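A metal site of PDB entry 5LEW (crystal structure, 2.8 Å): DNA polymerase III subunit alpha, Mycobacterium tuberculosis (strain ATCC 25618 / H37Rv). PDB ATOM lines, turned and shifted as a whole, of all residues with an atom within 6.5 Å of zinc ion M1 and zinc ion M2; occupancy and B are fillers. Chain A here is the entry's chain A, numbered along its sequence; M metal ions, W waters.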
ATOM      1  N   HIS A   8      19.818 -19.225  20.441  1.00  0.00           N
ATOM      2  CA  HIS A   8      18.642 -19.610  19.669  1.00  0.00           C
ATOM      3  C   HIS A   8      17.416 -18.815  20.099  1.00  0.00           C
ATOM      4  O   HIS A   8      16.890 -18.973  21.187  1.00  0.00           O
ATOM      5  CB  HIS A   8      18.413 -21.091  19.862  1.00  0.00           C
ATOM      6  CG  HIS A   8      17.370 -21.661  18.964  1.00  0.00           C
ATOM      7  ND1 HIS A   8      17.486 -22.927  18.426  1.00  0.00           N
ATOM      8  CD2 HIS A   8      16.214 -21.140  18.484  1.00  0.00           C
ATOM      9  CE1 HIS A   8      16.426 -23.175  17.672  1.00  0.00           C
ATOM     10  NE2 HIS A   8      15.669 -22.091  17.667  1.00  0.00           N
ATOM     11  N   ASN A   9      16.936 -17.966  19.201  1.00  0.00           N
ATOM     12  CA  ASN A   9      15.949 -16.921  19.550  1.00  0.00           C
ATOM     13  C   ASN A   9      15.050 -16.447  18.439  1.00  0.00           C
ATOM     14  O   ASN A   9      15.538 -16.116  17.368  1.00  0.00           O
ATOM     15  CB  ASN A   9      16.702 -15.675  19.846  1.00  0.00           C
ATOM     16  CG  ASN A   9      16.869 -15.491  21.237  1.00  0.00           C
ATOM     17  OD1 ASN A   9      15.888 -15.404  21.922  1.00  0.00           O
ATOM     18  ND2 ASN A   9      18.099 -15.424  21.707  1.00  0.00           N
ATOM     19  N   HIS A  10      13.751 -16.309  18.722  1.00  0.00           N
ATOM     20  CA  HIS A  10      12.784 -15.907  17.688  1.00  0.00           C
ATOM     21  C   HIS A  10      12.148 -14.560  17.917  1.00  0.00           C
ATOM     22  O   HIS A  10      11.444 -14.344  18.879  1.00  0.00           O
ATOM     23  CB  HIS A  10      11.742 -16.962  17.472  1.00  0.00           C
ATOM     24  CG  HIS A  10      12.298 -18.261  16.999  1.00  0.00           C
ATOM     25  ND1 HIS A  10      12.311 -18.611  15.682  1.00  0.00           N
ATOM     26  CD2 HIS A  10      12.880 -19.293  17.681  1.00  0.00           C
ATOM     27  CE1 HIS A  10      12.832 -19.830  15.557  1.00  0.00           C
ATOM     28  NE2 HIS A  10      13.207 -20.250  16.752  1.00  0.00           N
ATOM     29  N   THR A  40      17.624 -15.849  15.532  1.00  0.00           N
ATOM     30  CA  THR A  40      17.518 -17.129  14.828  1.00  0.00           C
ATOM     31  C   THR A  40      16.130 -17.282  14.251  1.00  0.00           C
ATOM     32  O   THR A  40      15.331 -18.072  14.737  1.00  0.00           O
ATOM     33  CB  THR A  40      17.850 -18.250  15.841  1.00  0.00           C
ATOM     34  OG1 THR A  40      19.236 -18.297  15.904  1.00  0.00           O
ATOM     35  CG2 THR A  40      17.467 -19.582  15.333  1.00  0.00           C
ATOM     36  N   HIS A  42      12.769 -18.117  11.879  1.00  0.00           N
ATOM     37  CA  HIS A  42      12.409 -19.275  11.091  1.00  0.00           C
ATOM     38  C   HIS A  42      12.473 -18.927   9.635  1.00  0.00           C
ATOM     39  O   HIS A  42      11.629 -18.244   9.106  1.00  0.00           O
ATOM     40  CB  HIS A  42      10.989 -19.723  11.387  1.00  0.00           C
ATOM     41  CG  HIS A  42      10.833 -20.447  12.678  1.00  0.00           C
ATOM     42  ND1 HIS A  42      11.425 -21.660  12.906  1.00  0.00           N
ATOM     43  CD2 HIS A  42      10.131 -20.152  13.786  1.00  0.00           C
ATOM     44  CE1 HIS A  42      11.102 -22.079  14.113  1.00  0.00           C
ATOM     45  NE2 HIS A  42      10.318 -21.174  14.672  1.00  0.00           N
ATOM     46  N   GLU A  67      17.251 -19.791  11.887  1.00  0.00           N
ATOM     47  CA  GLU A  67      16.837 -21.170  11.939  1.00  0.00           C
ATOM     48  C   GLU A  67      16.314 -21.625  10.595  1.00  0.00           C
ATOM     49  O   GLU A  67      15.110 -21.511  10.310  1.00  0.00           O
ATOM     50  CB  GLU A  67      15.825 -21.422  13.031  1.00  0.00           C
ATOM     51  CG  GLU A  67      15.754 -22.906  13.379  1.00  0.00           C
ATOM     52  CD  GLU A  67      14.920 -23.200  14.600  1.00  0.00           C
ATOM     53  OE1 GLU A  67      14.295 -22.272  15.184  1.00  0.00           O
ATOM     54  OE2 GLU A  67      14.904 -24.415  14.930  1.00  0.00           O
ATOM     55  N   HIS A 101      14.354 -28.271  11.183  1.00  0.00           N
ATOM     56  CA  HIS A 101      15.077 -27.066  11.607  1.00  0.00           C
ATOM     57  C   HIS A 101      16.575 -27.209  11.671  1.00  0.00           C
ATOM     58  O   HIS A 101      17.081 -28.327  11.840  1.00  0.00           O
ATOM     59  CB  HIS A 101      14.658 -26.701  13.003  1.00  0.00           C
ATOM     60  CG  HIS A 101      13.231 -26.334  13.112  1.00  0.00           C
ATOM     61  ND1 HIS A 101      12.712 -25.842  14.276  1.00  0.00           N
ATOM     62  CD2 HIS A 101      12.207 -26.412  12.216  1.00  0.00           C
ATOM     63  CE1 HIS A 101      11.420 -25.602  14.104  1.00  0.00           C
ATOM     64  NE2 HIS A 101      11.088 -25.946  12.861  1.00  0.00           N
ATOM     65  N   LEU A 102      17.302 -26.095  11.541  1.00  0.00           N
ATOM     66  CA  LEU A 102      18.723 -26.065  11.743  1.00  0.00           C
ATOM     67  C   LEU A 102      19.120 -24.696  12.239  1.00  0.00           C
ATOM     68  O   LEU A 102      18.828 -23.711  11.572  1.00  0.00           O
ATOM     69  CB  LEU A 102      19.412 -26.363  10.423  1.00  0.00           C
ATOM     70  CG  LEU A 102      20.949 -26.412  10.524  1.00  0.00           C
ATOM     71  CD1 LEU A 102      21.385 -27.441  11.560  1.00  0.00           C
ATOM     72  CD2 LEU A 102      21.642 -26.584   9.176  1.00  0.00           C
ATOM     73  N   THR A 103      19.778 -24.645  13.377  1.00  0.00           N
ATOM     74  CA  THR A 103      20.170 -23.368  14.006  1.00  0.00           C
ATOM     75  C   THR A 103      21.502 -22.986  13.396  1.00  0.00           C
ATOM     76  O   THR A 103      22.443 -23.780  13.518  1.00  0.00           O
ATOM     77  CB  THR A 103      20.403 -23.617  15.488  1.00  0.00           C
ATOM     78  OG1 THR A 103      19.347 -24.464  15.952  1.00  0.00           O
ATOM     79  CG2 THR A 103      20.474 -22.342  16.321  1.00  0.00           C
ATOM     80  N   GLY A 151      20.644 -29.051  16.500  1.00  0.00           N
ATOM     81  CA  GLY A 151      19.293 -28.567  16.380  1.00  0.00           C
ATOM     82  C   GLY A 151      18.355 -28.817  17.520  1.00  0.00           C
ATOM     83  O   GLY A 151      18.688 -29.586  18.429  1.00  0.00           O
ATOM     84  N   CYS A 152      17.215 -28.114  17.466  1.00  0.00           N
ATOM     85  CA  CYS A 152      16.035 -28.234  18.302  1.00  0.00           C
ATOM     86  C   CYS A 152      15.372 -29.604  18.071  1.00  0.00           C
ATOM     87  O   CYS A 152      15.822 -30.382  17.237  1.00  0.00           O
ATOM     88  CB  CYS A 152      15.044 -27.084  17.961  1.00  0.00           C
ATOM     89  SG  CYS A 152      13.969 -27.274  16.492  1.00  0.00           S
ATOM     90  N   PRO A 153      14.280 -29.908  18.784  1.00  0.00           N
ATOM     91  CA  PRO A 153      13.625 -31.170  18.483  1.00  0.00           C
ATOM     92  C   PRO A 153      13.158 -31.297  17.062  1.00  0.00           C
ATOM     93  O   PRO A 153      13.202 -32.368  16.537  1.00  0.00           O
ATOM     94  CB  PRO A 153      12.413 -31.189  19.394  1.00  0.00           C
ATOM     95  CG  PRO A 153      12.864 -30.338  20.546  1.00  0.00           C
ATOM     96  CD  PRO A 153      13.743 -29.271  19.988  1.00  0.00           C
ATOM     97  N   SER A 154      12.731 -30.244  16.391  1.00  0.00           N
ATOM     98  CA  SER A 154      12.349 -30.414  14.996  1.00  0.00           C
ATOM     99  C   SER A 154      13.551 -30.512  14.068  1.00  0.00           C
ATOM    100  O   SER A 154      13.365 -30.540  12.833  1.00  0.00           O
ATOM    101  CB  SER A 154      11.490 -29.257  14.547  1.00  0.00           C
ATOM    102  OG  SER A 154      10.192 -29.360  15.022  1.00  0.00           O
ATOM    103  N   GLY A 155      14.761 -30.510  14.630  1.00  0.00           N
ATOM    104  CA  GLY A 155      15.965 -30.843  13.870  1.00  0.00           C
ATOM    105  C   GLY A 155      16.060 -32.318  13.397  1.00  0.00           C
ATOM    106  O   GLY A 155      15.307 -33.174  13.864  1.00  0.00           O
ATOM    107  N   MET A 190      18.391 -28.300  25.140  1.00  0.00           N
ATOM    108  CA  MET A 190      17.264 -27.454  25.350  1.00  0.00           C
ATOM    109  C   MET A 190      16.432 -28.150  26.411  1.00  0.00           C
ATOM    110  O   MET A 190      16.044 -29.355  26.263  1.00  0.00           O
ATOM    111  CB  MET A 190      16.552 -27.525  24.028  1.00  0.00           C
ATOM    112  CG  MET A 190      15.406 -26.589  23.792  1.00  0.00           C
ATOM    113  SD  MET A 190      15.065 -26.468  22.021  1.00  0.00           S
ATOM    114  CE  MET A 190      16.564 -25.618  21.413  1.00  0.00           C
ATOM    115  N   ASP A 220      15.590 -21.428  22.721  1.00  0.00           N
ATOM    116  CA  ASP A 220      14.573 -21.370  21.654  1.00  0.00           C
ATOM    117  C   ASP A 220      13.457 -20.348  22.068  1.00  0.00           C
ATOM    118  O   ASP A 220      12.255 -20.636  22.032  1.00  0.00           O
ATOM    119  CB  ASP A 220      13.920 -22.777  21.472  1.00  0.00           C
ATOM    120  CG  ASP A 220      13.452 -23.031  20.049  1.00  0.00           C
ATOM    121  OD1 ASP A 220      13.650 -22.127  19.192  1.00  0.00           O
ATOM    122  OD2 ASP A 220      12.966 -24.147  19.765  1.00  0.00           O
ATOM    123  N   CYS A 221      13.886 -19.196  22.536  1.00  0.00           N
ATOM    124  CA  CYS A 221      12.963 -18.207  23.037  1.00  0.00           C
ATOM    125  C   CYS A 221      12.044 -17.757  21.936  1.00  0.00           C
ATOM    126  O   CYS A 221      12.518 -17.385  20.874  1.00  0.00           O
ATOM    127  CB  CYS A 221      13.723 -16.997  23.577  1.00  0.00           C
ATOM    128  SG  CYS A 221      15.147 -17.444  24.615  1.00  0.00           S
ATOM    129  N   HIS A 222      10.741 -17.837  22.185  1.00  0.00           N
ATOM    130  CA  HIS A 222       9.736 -17.290  21.300  1.00  0.00           C
ATOM    131  C   HIS A 222       9.059 -16.029  21.907  1.00  0.00           C
ATOM    132  O   HIS A 222       8.194 -15.444  21.284  1.00  0.00           O
ATOM    133  CB  HIS A 222       8.723 -18.379  20.921  1.00  0.00           C
ATOM    134  CG  HIS A 222       9.170 -19.302  19.815  1.00  0.00           C
ATOM    135  ND1 HIS A 222      10.023 -20.366  20.030  1.00  0.00           N
ATOM    136  CD2 HIS A 222       8.856 -19.337  18.494  1.00  0.00           C
ATOM    137  CE1 HIS A 222      10.247 -20.984  18.875  1.00  0.00           C
ATOM    138  NE2 HIS A 222       9.564 -20.382  17.930  1.00  0.00           N
HETATM  139 ZN    ZN M   1      13.429 -25.024  16.038  1.00  0.00          ZN
HETATM  140 ZN    ZN M   2      13.716 -22.244  17.152  1.00  0.00          ZN
HETATM  141 ZN    ZN M   3       9.087 -21.421  16.343  1.00  0.00          ZN
HETATM  142  O   HOH W   1      11.585 -23.244  17.015  1.00  0.00           O
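OE2 of Glu 67 binds zinc ion M1 (1.9 Å).
Zinc ion M1 is bound by a ring nitrogen (ND1) of His 101 (2.1 Å).
Zinc ion M1 is bound by SG of Cys 152 (2.4 Å).
Slightly farther from zinc ion M1 lies water W1 (2.7 Å).
Zinc ion M2 is bound by NE2 of His 8 (2.0 Å), OD1 of Asp 220 (2.0 Å), OE1 of Glu 67 (2.1 Å), NE2 of His 10 (2.1 Å) and water W1 (2.4 Å).
Zinc ion M2 has five donor atoms within binding distance.
A ring nitrogen (ND1) of His 10 sits close to the backbone carbonyl oxygen (O) of Thr 40, 3.2 Å away.
The backbone NH (N) of His 10 is in hydrogen-bond range of the backbone carbonyl oxygen (O) of Cys 221, at 2.7 Å.
The backbone carbonyl oxygen (O) of Asp 220 sits at hydrogen-bond distance from a ring nitrogen (ND1) of His 222.
N of Cys 221 is in hydrogen-bond range of O of His 8 (3.3 Å).
OG1 of Thr 103 sits at hydrogen-bond distance from ND1 of His 8, 3.5 Å away.
The backbone carbonyl oxygen (O) of Ser 154 is in hydrogen-bond range of the backbone NH (N) of His 101, 3.0 Å away.
The backbone NH of Ser 154 lies close to the side-chain sulfur of Cys 152 (3.2 Å).
A ring nitrogen (NE2) of His 42 lies close to a ring nitrogen (ND1) of His 10 (3.4 Å).
Within 4 Å of zinc ion M2: His 8, His 10, Glu 67 and Asp 220.
The nearest printed residue that does not touch zinc ion M2 is His 42 (4.01 Å).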
